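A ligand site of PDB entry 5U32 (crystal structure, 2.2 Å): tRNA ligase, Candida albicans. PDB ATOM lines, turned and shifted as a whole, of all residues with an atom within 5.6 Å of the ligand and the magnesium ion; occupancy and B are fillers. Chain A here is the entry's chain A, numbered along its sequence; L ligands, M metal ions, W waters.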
ATOM      1  N   THR A  21      11.834 -32.185  21.742  1.00  0.00           N
ATOM      2  CA  THR A  21      12.967 -31.890  20.885  1.00  0.00           C
ATOM      3  C   THR A  21      14.108 -31.366  21.755  1.00  0.00           C
ATOM      4  O   THR A  21      13.983 -31.244  22.983  1.00  0.00           O
ATOM      5  CB  THR A  21      12.598 -30.909  19.782  1.00  0.00           C
ATOM      6  OG1 THR A  21      12.281 -29.631  20.356  1.00  0.00           O
ATOM      7  CG2 THR A  21      11.418 -31.449  18.987  1.00  0.00           C
ATOM      8  N   ILE A  22      15.250 -31.055  21.121  1.00  0.00           N
ATOM      9  CA  ILE A  22      16.441 -30.696  21.879  1.00  0.00           C
ATOM     10  C   ILE A  22      16.197 -29.406  22.644  1.00  0.00           C
ATOM     11  O   ILE A  22      15.550 -28.473  22.141  1.00  0.00           O
ATOM     12  CB  ILE A  22      17.656 -30.582  20.947  1.00  0.00           C
ATOM     13  CG1 ILE A  22      17.945 -31.931  20.279  1.00  0.00           C
ATOM     14  CG2 ILE A  22      18.883 -30.080  21.699  1.00  0.00           C
ATOM     15  CD1 ILE A  22      19.063 -31.898  19.242  1.00  0.00           C
ATOM     16  N   GLY A  23      16.693 -29.358  23.880  1.00  0.00           N
ATOM     17  CA  GLY A  23      16.641 -28.160  24.674  1.00  0.00           C
ATOM     18  C   GLY A  23      15.312 -27.854  25.319  1.00  0.00           C
ATOM     19  O   GLY A  23      15.140 -26.755  25.849  1.00  0.00           O
ATOM     20  N   CYS A  24      14.358 -28.794  25.295  1.00  0.00           N
ATOM     21  CA  CYS A  24      13.079 -28.625  25.986  1.00  0.00           C
ATOM     22  C   CYS A  24      13.209 -28.712  27.506  1.00  0.00           C
ATOM     23  O   CYS A  24      12.251 -28.348  28.210  1.00  0.00           O
ATOM     24  CB  CYS A  24      12.093 -29.691  25.502  1.00  0.00           C
ATOM     25  SG  CYS A  24      11.359 -29.381  23.873  1.00  0.00           S
ATOM     26  N   GLY A  25      14.346 -29.173  28.018  1.00  0.00           N
ATOM     27  CA  GLY A  25      14.535 -29.347  29.440  1.00  0.00           C
ATOM     28  C   GLY A  25      14.524 -30.779  29.938  1.00  0.00           C
ATOM     29  O   GLY A  25      14.472 -30.978  31.154  1.00  0.00           O
ATOM     30  N   LYS A  26      14.607 -31.784  29.042  1.00  0.00           N
ATOM     31  CA  LYS A  26      14.555 -33.189  29.454  1.00  0.00           C
ATOM     32  C   LYS A  26      15.586 -33.512  30.521  1.00  0.00           C
ATOM     33  O   LYS A  26      15.265 -34.079  31.563  1.00  0.00           O
ATOM     34  CB  LYS A  26      14.787 -34.117  28.274  1.00  0.00           C
ATOM     35  CG  LYS A  26      13.691 -34.270  27.283  1.00  0.00           C
ATOM     36  CD  LYS A  26      14.111 -35.348  26.276  1.00  0.00           C
ATOM     37  CE  LYS A  26      15.519 -35.105  25.699  1.00  0.00           C
ATOM     38  NZ  LYS A  26      15.585 -33.921  24.741  1.00  0.00           N
ATOM     39  N   THR A  27      16.844 -33.206  30.247  1.00  0.00           N
ATOM     40  CA  THR A  27      17.894 -33.650  31.154  1.00  0.00           C
ATOM     41  C   THR A  27      17.852 -32.881  32.458  1.00  0.00           C
ATOM     42  O   THR A  27      18.085 -33.449  33.541  1.00  0.00           O
ATOM     43  CB  THR A  27      19.254 -33.553  30.476  1.00  0.00           C
ATOM     44  OG1 THR A  27      19.239 -34.404  29.327  1.00  0.00           O
ATOM     45  CG2 THR A  27      20.372 -34.026  31.399  1.00  0.00           C
ATOM     46  N   THR A  28      17.508 -31.586  32.393  1.00  0.00           N
ATOM     47  CA  THR A  28      17.384 -30.781  33.610  1.00  0.00           C
ATOM     48  C   THR A  28      16.263 -31.308  34.489  1.00  0.00           C
ATOM     49  O   THR A  28      16.421 -31.466  35.705  1.00  0.00           O
ATOM     50  CB  THR A  28      17.148 -29.314  33.239  1.00  0.00           C
ATOM     51  OG1 THR A  28      18.234 -28.861  32.430  1.00  0.00           O
ATOM     52  CG2 THR A  28      17.025 -28.440  34.505  1.00  0.00           C
ATOM     53  N   VAL A  29      15.119 -31.622  33.886  1.00  0.00           N
ATOM     54  CA  VAL A  29      13.986 -32.127  34.660  1.00  0.00           C
ATOM     55  C   VAL A  29      14.298 -33.509  35.241  1.00  0.00           C
ATOM     56  O   VAL A  29      14.065 -33.764  36.430  1.00  0.00           O
ATOM     57  CB  VAL A  29      12.724 -32.132  33.780  1.00  0.00           C
ATOM     58  CG1 VAL A  29      11.629 -32.939  34.430  1.00  0.00           C
ATOM     59  CG2 VAL A  29      12.262 -30.674  33.525  1.00  0.00           C
ATOM     60  N   GLN A  44      20.593 -41.845  29.980  1.00  0.00           N
ATOM     61  CA  GLN A  44      20.696 -40.733  29.040  1.00  0.00           C
ATOM     62  C   GLN A  44      21.236 -41.250  27.712  1.00  0.00           C
ATOM     63  O   GLN A  44      22.405 -41.620  27.616  1.00  0.00           O
ATOM     64  CB  GLN A  44      21.617 -39.643  29.587  1.00  0.00           C
ATOM     65  CG  GLN A  44      21.199 -39.083  30.924  1.00  0.00           C
ATOM     66  CD  GLN A  44      22.229 -38.125  31.486  1.00  0.00           C
ATOM     67  OE1 GLN A  44      22.853 -38.400  32.516  1.00  0.00           O
ATOM     68  NE2 GLN A  44      22.442 -37.005  30.801  1.00  0.00           N
ATOM     69  N   ASP A  46      22.164 -39.660  25.255  1.00  0.00           N
ATOM     70  CA  ASP A  46      23.326 -38.862  24.900  1.00  0.00           C
ATOM     71  C   ASP A  46      24.630 -39.441  25.417  1.00  0.00           C
ATOM     72  O   ASP A  46      25.693 -39.047  24.950  1.00  0.00           O
ATOM     73  CB  ASP A  46      23.167 -37.444  25.445  1.00  0.00           C
ATOM     74  CG  ASP A  46      22.332 -36.562  24.552  1.00  0.00           C
ATOM     75  OD1 ASP A  46      22.257 -36.876  23.340  1.00  0.00           O
ATOM     76  OD2 ASP A  46      21.753 -35.558  25.039  1.00  0.00           O
ATOM     77  N   ASP A  75      15.874 -40.999  28.851  1.00  0.00           N
ATOM     78  CA  ASP A  75      16.271 -39.666  28.414  1.00  0.00           C
ATOM     79  C   ASP A  75      16.662 -39.650  26.935  1.00  0.00           C
ATOM     80  O   ASP A  75      17.839 -39.689  26.576  1.00  0.00           O
ATOM     81  CB  ASP A  75      17.413 -39.129  29.264  1.00  0.00           C
ATOM     82  CG  ASP A  75      17.536 -37.624  29.176  1.00  0.00           C
ATOM     83  OD1 ASP A  75      17.192 -37.058  28.108  1.00  0.00           O
ATOM     84  OD2 ASP A  75      17.947 -36.997  30.169  1.00  0.00           O
ATOM     85  N   ASN A  77      14.788 -37.894  22.991  1.00  0.00           N
ATOM     86  CA  ASN A  77      13.793 -36.938  22.523  1.00  0.00           C
ATOM     87  C   ASN A  77      12.466 -37.612  22.177  1.00  0.00           C
ATOM     88  O   ASN A  77      11.400 -37.171  22.626  1.00  0.00           O
ATOM     89  CB  ASN A  77      14.327 -36.164  21.317  1.00  0.00           C
ATOM     90  CG  ASN A  77      15.216 -35.002  21.727  1.00  0.00           C
ATOM     91  OD1 ASN A  77      14.802 -34.146  22.508  1.00  0.00           O
ATOM     92  ND2 ASN A  77      16.448 -34.987  21.241  1.00  0.00           N
ATOM     93  N   ARG A 129      17.867 -21.263  24.389  1.00  0.00           N
ATOM     94  CA  ARG A 129      18.360 -22.034  25.525  1.00  0.00           C
ATOM     95  C   ARG A 129      19.688 -22.693  25.197  1.00  0.00           C
ATOM     96  O   ARG A 129      20.607 -22.668  26.004  1.00  0.00           O
ATOM     97  CB  ARG A 129      17.346 -23.097  25.935  1.00  0.00           C
ATOM     98  CG  ARG A 129      16.346 -22.673  26.983  1.00  0.00           C
ATOM     99  CD  ARG A 129      15.460 -23.844  27.396  1.00  0.00           C
ATOM    100  NE  ARG A 129      14.228 -23.353  27.998  1.00  0.00           N
ATOM    101  CZ  ARG A 129      13.197 -24.111  28.307  1.00  0.00           C
ATOM    102  NH1 ARG A 129      13.231 -25.423  28.056  1.00  0.00           N
ATOM    103  NH2 ARG A 129      12.116 -23.555  28.850  1.00  0.00           N
ATOM    104  N   VAL A 130      19.790 -23.287  24.012  1.00  0.00           N
ATOM    105  CA  VAL A 130      20.952 -24.128  23.723  1.00  0.00           C
ATOM    106  C   VAL A 130      22.174 -23.279  23.368  1.00  0.00           C
ATOM    107  O   VAL A 130      23.293 -23.580  23.801  1.00  0.00           O
ATOM    108  CB  VAL A 130      20.613 -25.168  22.640  1.00  0.00           C
ATOM    109  CG1 VAL A 130      21.842 -25.957  22.204  1.00  0.00           C
ATOM    110  CG2 VAL A 130      19.570 -26.127  23.172  1.00  0.00           C
ATOM    111  N   SER A 182       7.659 -22.607  28.283  1.00  0.00           N
ATOM    112  CA  SER A 182       7.533 -21.161  28.271  1.00  0.00           C
ATOM    113  C   SER A 182       8.898 -20.521  28.395  1.00  0.00           C
ATOM    114  O   SER A 182       9.837 -21.111  28.921  1.00  0.00           O
ATOM    115  CB  SER A 182       6.657 -20.685  29.429  1.00  0.00           C
ATOM    116  OG  SER A 182       7.387 -20.855  30.651  1.00  0.00           O
ATOM    117  N   ASP A 184      10.856 -18.151  30.656  1.00  0.00           N
ATOM    118  CA  ASP A 184      10.705 -18.009  32.090  1.00  0.00           C
ATOM    119  C   ASP A 184      10.051 -16.673  32.391  1.00  0.00           C
ATOM    120  O   ASP A 184      10.327 -15.657  31.741  1.00  0.00           O
ATOM    121  CB  ASP A 184      12.087 -18.152  32.735  1.00  0.00           C
ATOM    122  CG  ASP A 184      12.859 -19.336  32.156  1.00  0.00           C
ATOM    123  OD1 ASP A 184      12.308 -20.467  32.113  1.00  0.00           O
ATOM    124  OD2 ASP A 184      14.009 -19.162  31.716  1.00  0.00           O
ATOM    125  N   LYS A 189      11.758 -20.693  36.274  1.00  0.00           N
ATOM    126  CA  LYS A 189      12.140 -21.476  35.107  1.00  0.00           C
ATOM    127  C   LYS A 189      11.044 -22.481  34.821  1.00  0.00           C
ATOM    128  O   LYS A 189      10.485 -23.075  35.736  1.00  0.00           O
ATOM    129  CB  LYS A 189      13.468 -22.204  35.356  1.00  0.00           C
ATOM    130  CG  LYS A 189      14.611 -21.307  35.769  1.00  0.00           C
ATOM    131  CD  LYS A 189      15.271 -20.702  34.554  1.00  0.00           C
ATOM    132  CE  LYS A 189      16.500 -19.866  34.931  1.00  0.00           C
ATOM    133  NZ  LYS A 189      16.185 -18.430  35.242  1.00  0.00           N
ATOM    134  N   SER A 190      10.689 -22.661  33.537  1.00  0.00           N
ATOM    135  CA  SER A 190       9.595 -23.583  33.281  1.00  0.00           C
ATOM    136  C   SER A 190       9.998 -25.022  33.584  1.00  0.00           C
ATOM    137  O   SER A 190       9.141 -25.816  33.990  1.00  0.00           O
ATOM    138  CB  SER A 190       9.030 -23.426  31.853  1.00  0.00           C
ATOM    139  OG  SER A 190       9.857 -23.941  30.838  1.00  0.00           O
ATOM    140  N   SER A 191      11.277 -25.369  33.502  1.00  0.00           N
ATOM    141  CA  SER A 191      11.677 -26.698  33.958  1.00  0.00           C
ATOM    142  C   SER A 191      11.387 -26.913  35.445  1.00  0.00           C
ATOM    143  O   SER A 191      11.058 -28.033  35.862  1.00  0.00           O
ATOM    144  CB  SER A 191      13.149 -26.944  33.667  1.00  0.00           C
ATOM    145  OG  SER A 191      13.382 -27.023  32.264  1.00  0.00           O
ATOM    146  N   LEU A 192      11.500 -25.871  36.262  1.00  0.00           N
ATOM    147  CA  LEU A 192      11.163 -26.040  37.673  1.00  0.00           C
ATOM    148  C   LEU A 192       9.646 -26.152  37.859  1.00  0.00           C
ATOM    149  O   LEU A 192       9.157 -26.968  38.658  1.00  0.00           O
ATOM    150  CB  LEU A 192      11.721 -24.879  38.507  1.00  0.00           C
ATOM    151  CG  LEU A 192      11.230 -24.803  39.968  1.00  0.00           C
ATOM    152  CD1 LEU A 192      11.481 -26.104  40.718  1.00  0.00           C
ATOM    153  CD2 LEU A 192      11.892 -23.640  40.687  1.00  0.00           C
ATOM    154  N   PHE A 223      16.561 -28.739  41.961  1.00  0.00           N
ATOM    155  CA  PHE A 223      16.497 -28.132  40.633  1.00  0.00           C
ATOM    156  C   PHE A 223      17.676 -27.199  40.418  1.00  0.00           C
ATOM    157  O   PHE A 223      18.329 -27.228  39.368  1.00  0.00           O
ATOM    158  CB  PHE A 223      15.173 -27.381  40.450  1.00  0.00           C
ATOM    159  CG  PHE A 223      15.085 -26.625  39.170  1.00  0.00           C
ATOM    160  CD1 PHE A 223      14.786 -27.275  37.975  1.00  0.00           C
ATOM    161  CD2 PHE A 223      15.338 -25.253  39.134  1.00  0.00           C
ATOM    162  CE1 PHE A 223      14.715 -26.560  36.777  1.00  0.00           C
ATOM    163  CE2 PHE A 223      15.267 -24.551  37.942  1.00  0.00           C
ATOM    164  CZ  PHE A 223      14.961 -25.207  36.767  1.00  0.00           C
ATOM    165  N   ALA A 226      20.452 -29.141  39.294  1.00  0.00           N
ATOM    166  CA  ALA A 226      20.330 -29.546  37.894  1.00  0.00           C
ATOM    167  C   ALA A 226      20.568 -28.370  36.959  1.00  0.00           C
ATOM    168  O   ALA A 226      21.295 -28.510  35.965  1.00  0.00           O
ATOM    169  CB  ALA A 226      18.955 -30.160  37.637  1.00  0.00           C
ATOM    170  N   LEU A 227      19.947 -27.215  37.245  1.00  0.00           N
ATOM    171  CA  LEU A 227      20.107 -26.047  36.383  1.00  0.00           C
ATOM    172  C   LEU A 227      21.577 -25.703  36.187  1.00  0.00           C
ATOM    173  O   LEU A 227      22.025 -25.490  35.055  1.00  0.00           O
ATOM    174  CB  LEU A 227      19.342 -24.846  36.950  1.00  0.00           C
ATOM    175  CG  LEU A 227      19.078 -23.684  35.982  1.00  0.00           C
ATOM    176  CD1 LEU A 227      18.191 -24.122  34.826  1.00  0.00           C
ATOM    177  CD2 LEU A 227      18.460 -22.442  36.673  1.00  0.00           C
HETATM  178  P1  LIG L   1      17.563 -31.335  26.782  1.00  0.00           P
HETATM  179  O1  LIG L   1      18.213 -32.179  27.833  1.00  0.00           O
HETATM  180  O2  LIG L   1      16.065 -31.532  26.584  1.00  0.00           O
HETATM  181  O3  LIG L   1      18.322 -31.186  25.489  1.00  0.00           O
HETATM  182  O4  LIG L   1      17.577 -29.887  27.501  1.00  0.00           O
HETATM  183  P2  LIG L   1      18.494 -29.557  28.784  1.00  0.00           P
HETATM  184  O5  LIG L   1      19.901 -30.017  28.577  1.00  0.00           O
HETATM  185  O6  LIG L   1      17.810 -29.979  30.070  1.00  0.00           O
HETATM  186  O7  LIG L   1      18.489 -27.943  28.679  1.00  0.00           O
HETATM  187  C1  LIG L   1      19.375 -27.269  27.780  1.00  0.00           C
HETATM  188  C2  LIG L   1      19.815 -25.918  28.334  1.00  0.00           C
HETATM  189  O8  LIG L   1      18.678 -25.154  28.780  1.00  0.00           O
HETATM  190  C3  LIG L   1      20.712 -26.122  29.554  1.00  0.00           C
HETATM  191  O9  LIG L   1      21.769 -25.146  29.501  1.00  0.00           O
HETATM  192  C4  LIG L   1      19.779 -25.876  30.731  1.00  0.00           C
HETATM  193  O10 LIG L   1      20.449 -25.377  31.889  1.00  0.00           O
HETATM  194  C5  LIG L   1      18.783 -24.879  30.182  1.00  0.00           C
HETATM  195  N1  LIG L   1      17.438 -24.976  30.797  1.00  0.00           N
HETATM  196  C6  LIG L   1      16.802 -26.071  31.258  1.00  0.00           C
HETATM  197  N2  LIG L   1      15.572 -25.763  31.751  1.00  0.00           N
HETATM  198  C7  LIG L   1      15.418 -24.435  31.599  1.00  0.00           C
HETATM  199  C8  LIG L   1      14.354 -23.461  31.918  1.00  0.00           C
HETATM  200  O11 LIG L   1      13.284 -23.827  32.444  1.00  0.00           O
HETATM  201  N3  LIG L   1      14.591 -22.179  31.617  1.00  0.00           N
HETATM  202  C9  LIG L   1      15.752 -21.775  31.035  1.00  0.00           C
HETATM  203  N4  LIG L   1      15.915 -20.460  30.762  1.00  0.00           N
HETATM  204  N5  LIG L   1      16.777 -22.607  30.712  1.00  0.00           N
HETATM  205  C10 LIG L   1      16.654 -23.932  30.986  1.00  0.00           C
HETATM  206 MG    MG M   1      19.920 -33.614  27.433  1.00  0.00          MG
HETATM  207  O   HOH W   1      15.390 -17.198  30.587  1.00  0.00           O
HETATM  208  O   HOH W   2      18.494 -35.151  26.643  1.00  0.00           O
HETATM  209  O   HOH W   3      17.867 -19.519  28.937  1.00  0.00           O
HETATM  210  O   HOH W   4      21.319 -32.233  27.916  1.00  0.00           O
HETATM  211  O   HOH W   5      20.842 -27.823  33.218  1.00  0.00           O
HETATM  212  O   HOH W   6      20.418 -33.165  25.436  1.00  0.00           O
HETATM  213  O   HOH W   7      21.261 -35.353  27.557  1.00  0.00           O
HETATM  214  O   HOH W   8      13.664 -20.686  28.372  1.00  0.00           O
HETATM  215  O   HOH W   9      18.159 -33.253  23.477  1.00  0.00           O
HETATM  216  O   HOH W  10      21.061 -29.809  24.971  1.00  0.00           O
HETATM  217  O   HOH W  11      23.816 -25.088  31.248  1.00  0.00           O
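The backbone NH of Gly 23 sits at hydrogen-bond distance from an oxygen (O3) of the ligand (2.9 Å). NZ of Lys 26 lies within salt-bridge range of O2 of the ligand (3.1 Å). The backbone NH of Lys 26 is in hydrogen-bond range of an oxygen (O2) of the ligand. The backbone NH (N) of Thr 27 lies within hydrogen-bond range of an oxygen (O6) of the ligand (3.4 Å). An oxygen (O11) of the ligand lies within hydrogen-bond range of the backbone NH (N) of Ser 190 (3.0 Å). The side-chain carboxylate (OD2) of Asp 184 is in hydrogen-bond range of a nitrogen (N4) of the ligand. O2 of the ligand lies within hydrogen-bond range of N of Gly 25 (3.3 Å). The side-chain hydroxyl of Ser 191 sits at hydrogen-bond distance from a nitrogen (N2) of the ligand, at 2.6 Å. The backbone NH (N) of Cys 24 is in hydrogen-bond range of an oxygen (O2) of the ligand, at 3.5 Å. The side-chain hydroxyl (OG1) of Thr 28 sits at hydrogen-bond distance from an oxygen (O6) of the ligand, at 2.6 Å. An oxygen (O11) of the ligand sits at hydrogen-bond distance from the backbone NH (N) of Ser 191 (2.7 Å). The backbone NH (N) of Thr 28 sits at hydrogen-bond distance from an oxygen (O6) of the ligand, 2.8 Å away.
The guanidinium group of Arg 129 sits at hydrogen-bond distance from the side-chain hydroxyl of Ser 190 (3.0 Å). O of Gly 23 is in hydrogen-bond range of NH1 of Arg 129 (3.2 Å). The side-chain hydroxyl (OG) of Ser 190 is in hydrogen-bond range of the backbone carbonyl oxygen (O) of Ser 182 (3.4 Å). The backbone NH of Ser 190 lies within hydrogen-bond range of the side-chain carboxylate of Asp 184 (3.1 Å). OG1 of Thr 27 lies close to OD2 of Asp 75, at 3.0 Å. NH2 of Arg 129 sits at hydrogen-bond distance from O of Ser 182, 3.3 Å away. The backbone carbonyl oxygen (O) of Cys 24 is in hydrogen-bond range of the guanidinium group (NH1) of Arg 129, at 3.1 Å. The side-chain sulfur (SG) of Cys 24 is in hydrogen-bond range of the backbone carbonyl oxygen (O) of Thr 21 (3.3 Å).
C of Ile 22 touches O3 of the ligand, 3.97 Å away. CD of Arg 129 touches O8 of the ligand, at 3.7 Å. Lys 189 touches the ligand (CB to O11, 3.3 Å). Leu 227 touches the ligand. Hydrophobic or aromatic side chains within 4 Å of the ligand: Ile 22 and Leu 227. The nearest printed residue that does not touch the ligand is Thr 21 (4.2 Å).
Merely in contact with the magnesium ion: Asp 46. Of the 24 residues printed, 2 come within 4 Å of the magnesium ion.
The magnesium ion is bound by water W4 (2.0 Å), water W6 (2.1 Å), OG1 of Thr 27 (2.2 Å), water W7 (2.2 Å), water W2 (2.2 Å) and O1 of the ligand (2.3 Å). The magnesium ion has six donor atoms within binding distance.
Water W6 bridges OD2 of Asp 46 and O3 of the ligand. Water W5 lies within hydrogen-bond range of O10 of the ligand (2.8 Å), O of Ala 226 (2.9 Å), OG1 of Thr 28 (2.9 Å) and O of Leu 227 (3.2 Å). Water W9 lies within hydrogen-bond range of O3 of the ligand, NZ of Lys 26 and ND2 of Asn 77. Water W8 lies within hydrogen-bond range of the guanidinium group (NE) of Arg 129 (2.8 Å) and a nitrogen (N4) of the ligand (3.3 Å). Water W1 lies within hydrogen-bond range of OD2 of Asp 184 (2.7 Å) and N4 of the ligand (3.3 Å).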
